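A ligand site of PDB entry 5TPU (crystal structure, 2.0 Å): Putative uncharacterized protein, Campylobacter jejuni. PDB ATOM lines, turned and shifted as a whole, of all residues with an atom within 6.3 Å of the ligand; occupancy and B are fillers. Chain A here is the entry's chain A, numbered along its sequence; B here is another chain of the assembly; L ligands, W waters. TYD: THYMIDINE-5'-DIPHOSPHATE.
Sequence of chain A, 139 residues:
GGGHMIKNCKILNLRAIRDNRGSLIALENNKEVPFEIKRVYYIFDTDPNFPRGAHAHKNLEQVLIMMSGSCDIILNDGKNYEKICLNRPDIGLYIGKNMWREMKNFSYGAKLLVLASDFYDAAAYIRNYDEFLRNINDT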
ATOM      1  N   ARG A  39       2.678  26.160 -15.283  1.00  0.00           N
ATOM      2  CA  ARG A  39       2.221  25.303 -14.203  1.00  0.00           C
ATOM      3  C   ARG A  39       2.904  23.959 -14.379  1.00  0.00           C
ATOM      4  O   ARG A  39       3.094  23.453 -15.486  1.00  0.00           O
ATOM      5  CB  ARG A  39       0.694  25.196 -14.172  1.00  0.00           C
ATOM      6  CG  ARG A  39       0.201  24.093 -13.261  1.00  0.00           C
ATOM      7  CD  ARG A  39      -1.329  23.918 -13.170  1.00  0.00           C
ATOM      8  NE  ARG A  39      -2.025  24.073 -14.448  1.00  0.00           N
ATOM      9  CZ  ARG A  39      -3.081  23.381 -14.828  1.00  0.00           C
ATOM     10  NH1 ARG A  39      -3.637  23.636 -15.997  1.00  0.00           N
ATOM     11  NH2 ARG A  39      -3.604  22.436 -14.056  1.00  0.00           N
ATOM     12  N   VAL A  40       3.369  23.408 -13.258  1.00  0.00           N
ATOM     13  CA  VAL A  40       3.876  22.071 -13.238  1.00  0.00           C
ATOM     14  C   VAL A  40       3.080  21.440 -12.135  1.00  0.00           C
ATOM     15  O   VAL A  40       2.868  22.006 -11.056  1.00  0.00           O
ATOM     16  CB  VAL A  40       5.393  22.050 -12.951  1.00  0.00           C
ATOM     17  CG1 VAL A  40       5.877  20.626 -12.731  1.00  0.00           C
ATOM     18  CG2 VAL A  40       6.169  22.663 -14.090  1.00  0.00           C
ATOM     19  N   TYR A  41       2.573  20.257 -12.398  1.00  0.00           N
ATOM     20  CA  TYR A  41       1.954  19.503 -11.318  1.00  0.00           C
ATOM     21  C   TYR A  41       2.310  18.039 -11.397  1.00  0.00           C
ATOM     22  O   TYR A  41       2.758  17.536 -12.454  1.00  0.00           O
ATOM     23  CB  TYR A  41       0.441  19.738 -11.329  1.00  0.00           C
ATOM     24  CG  TYR A  41      -0.367  19.178 -12.479  1.00  0.00           C
ATOM     25  CD1 TYR A  41      -0.934  17.922 -12.396  1.00  0.00           C
ATOM     26  CD2 TYR A  41      -0.611  19.929 -13.638  1.00  0.00           C
ATOM     27  CE1 TYR A  41      -1.687  17.422 -13.429  1.00  0.00           C
ATOM     28  CE2 TYR A  41      -1.398  19.428 -14.685  1.00  0.00           C
ATOM     29  CZ  TYR A  41      -1.941  18.183 -14.560  1.00  0.00           C
ATOM     30  OH  TYR A  41      -2.701  17.594 -15.520  1.00  0.00           O
ATOM     31  N   ILE A  43       1.301  13.960  -9.804  1.00  0.00           N
ATOM     32  CA  ILE A  43       0.373  13.060  -9.149  1.00  0.00           C
ATOM     33  C   ILE A  43       1.153  11.834  -8.687  1.00  0.00           C
ATOM     34  O   ILE A  43       2.004  11.312  -9.407  1.00  0.00           O
ATOM     35  CB  ILE A  43      -0.766  12.647 -10.068  1.00  0.00           C
ATOM     36  CG1 ILE A  43      -1.545  13.880 -10.518  1.00  0.00           C
ATOM     37  CG2 ILE A  43      -1.722  11.732  -9.368  1.00  0.00           C
ATOM     38  CD1 ILE A  43      -2.472  13.673 -11.697  1.00  0.00           C
ATOM     39  N   ARG A  52      -8.593   8.049 -13.016  1.00  0.00           N
ATOM     40  CA  ARG A  52      -8.987   9.431 -13.000  1.00  0.00           C
ATOM     41  C   ARG A  52     -10.198   9.603 -13.880  1.00  0.00           C
ATOM     42  O   ARG A  52     -10.610   8.691 -14.600  1.00  0.00           O
ATOM     43  CB  ARG A  52      -7.830  10.268 -13.451  1.00  0.00           C
ATOM     44  CG  ARG A  52      -6.595   9.869 -12.697  1.00  0.00           C
ATOM     45  CD  ARG A  52      -5.587  10.987 -12.683  1.00  0.00           C
ATOM     46  NE  ARG A  52      -5.978  12.062 -11.792  1.00  0.00           N
ATOM     47  CZ  ARG A  52      -5.814  12.083 -10.486  1.00  0.00           C
ATOM     48  NH1 ARG A  52      -6.167  13.170  -9.807  1.00  0.00           N
ATOM     49  NH2 ARG A  52      -5.292  11.045  -9.858  1.00  0.00           N
ATOM     50  N   GLY A  53     -10.811  10.771 -13.809  1.00  0.00           N
ATOM     51  CA  GLY A  53     -12.012  11.002 -14.618  1.00  0.00           C
ATOM     52  C   GLY A  53     -11.667  11.440 -16.027  1.00  0.00           C
ATOM     53  O   GLY A  53     -10.700  12.123 -16.237  1.00  0.00           O
ATOM     54  N   HIS A  55     -12.216  13.736 -19.203  1.00  0.00           N
ATOM     55  CA  HIS A  55     -12.672  15.089 -19.465  1.00  0.00           C
ATOM     56  C   HIS A  55     -11.864  15.622 -20.615  1.00  0.00           C
ATOM     57  O   HIS A  55     -10.872  14.994 -21.012  1.00  0.00           O
ATOM     58  CB  HIS A  55     -12.471  15.964 -18.241  1.00  0.00           C
ATOM     59  CG  HIS A  55     -11.036  16.059 -17.811  1.00  0.00           C
ATOM     60  ND1 HIS A  55     -10.447  15.124 -17.003  1.00  0.00           N
ATOM     61  CD2 HIS A  55     -10.088  16.973 -18.090  1.00  0.00           C
ATOM     62  CE1 HIS A  55      -9.181  15.436 -16.812  1.00  0.00           C
ATOM     63  NE2 HIS A  55      -8.943  16.572 -17.453  1.00  0.00           N
ATOM     64  N   GLN A  62      -0.556  20.231 -22.540  1.00  0.00           N
ATOM     65  CA  GLN A  62       0.249  19.559 -21.525  1.00  0.00           C
ATOM     66  C   GLN A  62       1.326  18.647 -22.094  1.00  0.00           C
ATOM     67  O   GLN A  62       1.201  18.095 -23.186  1.00  0.00           O
ATOM     68  CB  GLN A  62      -0.640  18.721 -20.602  1.00  0.00           C
ATOM     69  CG  GLN A  62      -1.676  19.492 -19.788  1.00  0.00           C
ATOM     70  CD  GLN A  62      -2.848  18.589 -19.436  1.00  0.00           C
ATOM     71  OE1 GLN A  62      -3.524  18.052 -20.319  1.00  0.00           O
ATOM     72  NE2 GLN A  62      -3.059  18.371 -18.171  1.00  0.00           N
ATOM     73  N   PHE A 119      -2.521  28.114 -16.308  1.00  0.00           N
ATOM     74  CA  PHE A 119      -2.817  27.962 -14.892  1.00  0.00           C
ATOM     75  C   PHE A 119      -4.049  27.094 -14.666  1.00  0.00           C
ATOM     76  O   PHE A 119      -4.848  26.955 -15.563  1.00  0.00           O
ATOM     77  CB  PHE A 119      -3.057  29.347 -14.312  1.00  0.00           C
ATOM     78  CG  PHE A 119      -1.866  30.258 -14.427  1.00  0.00           C
ATOM     79  CD1 PHE A 119      -0.831  30.157 -13.525  1.00  0.00           C
ATOM     80  CD2 PHE A 119      -1.817  31.249 -15.403  1.00  0.00           C
ATOM     81  CE1 PHE A 119       0.275  30.997 -13.637  1.00  0.00           C
ATOM     82  CE2 PHE A 119      -0.742  32.111 -15.493  1.00  0.00           C
ATOM     83  CZ  PHE A 119       0.309  31.999 -14.603  1.00  0.00           C
ATOM     84  N   TYR A 120      -4.169  26.508 -13.478  1.00  0.00           N
ATOM     85  CA  TYR A 120      -5.287  25.607 -13.150  1.00  0.00           C
ATOM     86  C   TYR A 120      -6.583  26.391 -13.168  1.00  0.00           C
ATOM     87  O   TYR A 120      -6.612  27.516 -12.660  1.00  0.00           O
ATOM     88  CB  TYR A 120      -5.157  25.041 -11.745  1.00  0.00           C
ATOM     89  CG  TYR A 120      -6.400  24.279 -11.284  1.00  0.00           C
ATOM     90  CD1 TYR A 120      -6.722  23.061 -11.843  1.00  0.00           C
ATOM     91  CD2 TYR A 120      -7.217  24.779 -10.283  1.00  0.00           C
ATOM     92  CE1 TYR A 120      -7.858  22.355 -11.451  1.00  0.00           C
ATOM     93  CE2 TYR A 120      -8.349  24.093  -9.881  1.00  0.00           C
ATOM     94  CZ  TYR A 120      -8.681  22.884 -10.461  1.00  0.00           C
ATOM     95  OH  TYR A 120      -9.810  22.184 -10.041  1.00  0.00           O
ATOM     96  N   ASP A 121      -7.649  25.781 -13.683  1.00  0.00           N
ATOM     97  CA  ASP A 121      -8.970  26.394 -13.750  1.00  0.00           C
ATOM     98  C   ASP A 121     -10.043  25.290 -13.877  1.00  0.00           C
ATOM     99  O   ASP A 121     -10.164  24.617 -14.917  1.00  0.00           O
ATOM    100  CB  ASP A 121      -9.002  27.422 -14.893  1.00  0.00           C
ATOM    101  CG  ASP A 121     -10.407  27.961 -15.183  1.00  0.00           C
ATOM    102  OD1 ASP A 121     -11.305  27.865 -14.318  1.00  0.00           O
ATOM    103  OD2 ASP A 121     -10.603  28.444 -16.319  1.00  0.00           O
ATOM    104  N   TYR A 125     -12.538  22.360 -17.233  1.00  0.00           N
ATOM    105  CA  TYR A 125     -12.723  20.930 -17.452  1.00  0.00           C
ATOM    106  C   TYR A 125     -14.053  20.695 -18.131  1.00  0.00           C
ATOM    107  O   TYR A 125     -15.088  21.112 -17.638  1.00  0.00           O
ATOM    108  CB  TYR A 125     -12.710  20.136 -16.153  1.00  0.00           C
ATOM    109  CG  TYR A 125     -11.382  19.961 -15.474  1.00  0.00           C
ATOM    110  CD1 TYR A 125     -10.655  21.040 -14.981  1.00  0.00           C
ATOM    111  CD2 TYR A 125     -10.907  18.677 -15.224  1.00  0.00           C
ATOM    112  CE1 TYR A 125      -9.460  20.847 -14.296  1.00  0.00           C
ATOM    113  CE2 TYR A 125      -9.689  18.478 -14.571  1.00  0.00           C
ATOM    114  CZ  TYR A 125      -8.984  19.560 -14.095  1.00  0.00           C
ATOM    115  OH  TYR A 125      -7.811  19.314 -13.416  1.00  0.00           O
ATOM    116  N   ARG A 127     -16.491  17.859 -18.731  1.00  0.00           N
ATOM    117  CA  ARG A 127     -16.841  16.541 -18.276  1.00  0.00           C
ATOM    118  C   ARG A 127     -17.943  15.882 -19.060  1.00  0.00           C
ATOM    119  O   ARG A 127     -18.022  14.680 -19.030  1.00  0.00           O
ATOM    120  CB  ARG A 127     -17.234  16.655 -16.818  1.00  0.00           C
ATOM    121  CG  ARG A 127     -16.100  17.349 -16.093  1.00  0.00           C
ATOM    122  CD  ARG A 127     -16.027  16.917 -14.668  1.00  0.00           C
ATOM    123  NE  ARG A 127     -15.126  17.800 -13.949  1.00  0.00           N
ATOM    124  CZ  ARG A 127     -13.913  17.485 -13.490  1.00  0.00           C
ATOM    125  NH1 ARG A 127     -13.357  16.272 -13.696  1.00  0.00           N
ATOM    126  NH2 ARG A 127     -13.224  18.448 -12.853  1.00  0.00           N
ATOM    127  N   ILE B  17      -3.532  17.962  -2.849  1.00  0.00           N
ATOM    128  CA  ILE B  17      -4.889  17.417  -2.850  1.00  0.00           C
ATOM    129  C   ILE B  17      -4.828  15.880  -2.780  1.00  0.00           C
ATOM    130  O   ILE B  17      -4.192  15.286  -3.620  1.00  0.00           O
ATOM    131  CB  ILE B  17      -5.660  17.855  -4.099  1.00  0.00           C
ATOM    132  CG1 ILE B  17      -5.476  19.348  -4.406  1.00  0.00           C
ATOM    133  CG2 ILE B  17      -7.137  17.475  -3.992  1.00  0.00           C
ATOM    134  CD1 ILE B  17      -5.993  20.282  -3.356  1.00  0.00           C
ATOM    135  N   ASP B  19      -7.025  12.183  -2.429  1.00  0.00           N
ATOM    136  CA  ASP B  19      -8.341  11.578  -2.615  1.00  0.00           C
ATOM    137  C   ASP B  19      -8.002  10.154  -2.851  1.00  0.00           C
ATOM    138  O   ASP B  19      -6.837   9.774  -2.742  1.00  0.00           O
ATOM    139  CB  ASP B  19      -9.180  12.236  -3.753  1.00  0.00           C
ATOM    140  CG  ASP B  19      -8.458  12.287  -5.102  1.00  0.00           C
ATOM    141  OD1 ASP B  19      -7.822  11.300  -5.542  1.00  0.00           O
ATOM    142  OD2 ASP B  19      -8.492  13.325  -5.723  1.00  0.00           O
ATOM    143  N   ARG B  21      -7.717   8.484  -5.513  1.00  0.00           N
ATOM    144  CA  ARG B  21      -6.884   8.283  -6.696  1.00  0.00           C
ATOM    145  C   ARG B  21      -5.403   8.618  -6.489  1.00  0.00           C
ATOM    146  O   ARG B  21      -4.584   8.250  -7.287  1.00  0.00           O
ATOM    147  CB  ARG B  21      -7.403   9.129  -7.873  1.00  0.00           C
ATOM    148  CG  ARG B  21      -8.843   8.828  -8.257  1.00  0.00           C
ATOM    149  CD  ARG B  21      -9.427   9.864  -9.204  1.00  0.00           C
ATOM    150  NE  ARG B  21      -9.414  11.195  -8.579  1.00  0.00           N
ATOM    151  CZ  ARG B  21      -9.590  12.354  -9.189  1.00  0.00           C
ATOM    152  NH1 ARG B  21      -9.789  12.426 -10.501  1.00  0.00           N
ATOM    153  NH2 ARG B  21      -9.504  13.467  -8.458  1.00  0.00           N
ATOM    154  N   LEU B  24      -2.109  15.074  -5.565  1.00  0.00           N
ATOM    155  CA  LEU B  24      -1.667  16.017  -6.572  1.00  0.00           C
ATOM    156  C   LEU B  24      -1.145  17.281  -5.900  1.00  0.00           C
ATOM    157  O   LEU B  24      -1.769  17.855  -4.973  1.00  0.00           O
ATOM    158  CB  LEU B  24      -2.793  16.371  -7.525  1.00  0.00           C
ATOM    159  CG  LEU B  24      -2.553  17.280  -8.710  1.00  0.00           C
ATOM    160  CD1 LEU B  24      -3.457  16.890  -9.850  1.00  0.00           C
ATOM    161  CD2 LEU B  24      -2.664  18.762  -8.455  1.00  0.00           C
ATOM    162  N   ILE B  25      -0.005  17.713  -6.437  1.00  0.00           N
ATOM    163  CA  ILE B  25       0.565  18.989  -6.072  1.00  0.00           C
ATOM    164  C   ILE B  25       0.841  19.735  -7.351  1.00  0.00           C
ATOM    165  O   ILE B  25       1.322  19.171  -8.347  1.00  0.00           O
ATOM    166  CB  ILE B  25       1.883  18.841  -5.317  1.00  0.00           C
ATOM    167  CG1 ILE B  25       1.610  18.251  -3.928  1.00  0.00           C
ATOM    168  CG2 ILE B  25       2.594  20.201  -5.203  1.00  0.00           C
ATOM    169  CD1 ILE B  25       2.861  17.737  -3.254  1.00  0.00           C
ATOM    170  N   ALA B  26       0.553  21.035  -7.266  1.00  0.00           N
ATOM    171  CA  ALA B  26       0.690  21.900  -8.407  1.00  0.00           C
ATOM    172  C   ALA B  26       1.509  23.109  -7.996  1.00  0.00           C
ATOM    173  O   ALA B  26       1.320  23.650  -6.894  1.00  0.00           O
ATOM    174  CB  ALA B  26      -0.684  22.294  -8.909  1.00  0.00           C
ATOM    175  N   GLU B  28       2.713  26.901  -9.669  1.00  0.00           N
ATOM    176  CA  GLU B  28       2.415  27.847 -10.728  1.00  0.00           C
ATOM    177  C   GLU B  28       3.317  29.069 -10.635  1.00  0.00           C
ATOM    178  O   GLU B  28       3.764  29.486  -9.547  1.00  0.00           O
ATOM    179  CB  GLU B  28       0.923  28.212 -10.798  1.00  0.00           C
ATOM    180  CG  GLU B  28       0.032  27.024 -11.064  1.00  0.00           C
ATOM    181  CD  GLU B  28      -1.447  27.374 -11.084  1.00  0.00           C
ATOM    182  OE1 GLU B  28      -1.917  28.125 -10.216  1.00  0.00           O
ATOM    183  OE2 GLU B  28      -2.185  26.915 -11.952  1.00  0.00           O
HETATM  184  PA  TYD L   1      -8.062  16.379 -11.357  1.00  0.00           P
HETATM  185  O1A TYD L   1      -8.007  14.892 -11.151  1.00  0.00           O
HETATM  186  O2A TYD L   1      -7.369  17.088 -12.449  1.00  0.00           O
HETATM  187  O3A TYD L   1      -9.547  16.967 -11.402  1.00  0.00           O
HETATM  188  PB  TYD L   1     -10.897  16.243 -10.862  1.00  0.00           P
HETATM  189  O1B TYD L   1     -11.770  17.490 -10.632  1.00  0.00           O
HETATM  190  O2B TYD L   1     -10.504  15.585  -9.574  1.00  0.00           O
HETATM  191  O3B TYD L   1     -11.262  15.297 -11.968  1.00  0.00           O
HETATM  192  O5' TYD L   1      -7.275  17.024 -10.150  1.00  0.00           O
HETATM  193  C5' TYD L   1      -7.270  16.398  -8.864  1.00  0.00           C
HETATM  194  C4' TYD L   1      -7.447  17.453  -7.812  1.00  0.00           C
HETATM  195  O4' TYD L   1      -6.460  18.478  -7.871  1.00  0.00           O
HETATM  196  C3' TYD L   1      -8.761  18.146  -7.989  1.00  0.00           C
HETATM  197  O3' TYD L   1      -9.334  18.159  -6.669  1.00  0.00           O
HETATM  198  C2' TYD L   1      -8.411  19.497  -8.650  1.00  0.00           C
HETATM  199  C1' TYD L   1      -7.014  19.720  -8.121  1.00  0.00           C
HETATM  200  N1  TYD L   1      -6.059  20.324  -9.002  1.00  0.00           N
HETATM  201  C2  TYD L   1      -5.358  21.470  -8.566  1.00  0.00           C
HETATM  202  O2  TYD L   1      -5.595  21.951  -7.413  1.00  0.00           O
HETATM  203  N3  TYD L   1      -4.446  22.050  -9.361  1.00  0.00           N
HETATM  204  C4  TYD L   1      -4.132  21.558 -10.580  1.00  0.00           C
HETATM  205  O4  TYD L   1      -3.267  22.124 -11.269  1.00  0.00           O
HETATM  206  C5  TYD L   1      -4.835  20.340 -11.029  1.00  0.00           C
HETATM  207  C5M TYD L   1      -4.566  19.722 -12.358  1.00  0.00           C
HETATM  208  C6  TYD L   1      -5.766  19.758 -10.198  1.00  0.00           C
HETATM  209  O   HOH W   1      -9.872  13.595 -13.501  1.00  0.00           O
HETATM  210  O   HOH W   2     -12.816  13.304 -11.377  1.00  0.00           O
HETATM  211  O   HOH W   3     -14.244  16.915  -9.716  1.00  0.00           O
HETATM  212  O   HOH W   4      -6.088  14.553  -6.224  1.00  0.00           O
HETATM  213  O   HOH W   5      -9.839  15.772  -5.362  1.00  0.00           O
HETATM  214  O   HOH W   6      -3.116  24.736  -8.841  1.00  0.00           O
HETATM  215  O   HOH W   7     -10.850  20.019 -11.185  1.00  0.00           O
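Water W2 bridges O3B of the ligand (2.6 Å) and NH1 of Arg 21 of chain B (3.3 Å). Water W1 lies within hydrogen-bond range of an oxygen (O3B) of the ligand, the backbone NH (N) of Gly 53 and the guanidinium group (NH1) of Arg 21 of chain B. Water W7 lies within hydrogen-bond range of OH of Tyr 120, O1B of the ligand and NH2 of Arg 127. Water W5 lies within hydrogen-bond range of O3' of the ligand (2.8 Å) and OD2 of Asp 19 of chain B (2.8 Å). Water W4 bridges OD2 of Asp 19 of chain B (2.7 Å) and O of Ile 17 of chain B (3.3 Å).
The guanidinium group (NH2) of Arg 21 of chain B is in salt-bridge range of the side-chain carboxylate (OD2) of Asp 19 of chain B (2.9 Å). The guanidinium group (NE) of Arg 39 is in salt-bridge range of the side-chain carboxylate (OE2) of Glu 28 of chain B (3.8 Å). N of Tyr 120 is in hydrogen-bond range of OE2 of Glu 28 of chain B, at 2.5 Å. The backbone NH (N) of Ile 17 of chain B sits at hydrogen-bond distance from the backbone carbonyl oxygen (O) of Leu 24 of chain B. The side-chain amide nitrogen (NE2) of Gln 62 is in hydrogen-bond range of the side-chain hydroxyl (OH) of Tyr 41 (2.8 Å).
The side-chain hydroxyl of Tyr 125 sits at hydrogen-bond distance from an oxygen (O2A) of the ligand (2.5 Å). NH2 of Arg 21 of chain B is in salt-bridge range of O2B of the ligand, at 2.6 Å. The guanidinium group (NH2) of Arg 127 lies within salt-bridge range of an oxygen (O1B) of the ligand (2.8 Å). NH2 of Arg 39 sits at hydrogen-bond distance from O4 of the ligand, at 2.8 Å. NH1 of Arg 52 lies within salt-bridge range of O1A of the ligand, 2.9 Å away.
Merely in contact with the ligand: Tyr 120 (3.2 Å), Ala 26 of chain B (3.5 Å), Ile 17 of chain B (3.5 Å), Leu 24 of chain B (3.7 Å) and Tyr 41 (3.8 Å). Hydrophobic or aromatic side chains that line the ligand: Tyr 41, Tyr 120, Tyr 125, Ile 17 of chain B, Leu 24 of chain B and Ala 26 of chain B. Along chain A the residues within 4 Å of the ligand span positions 39 to 127.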
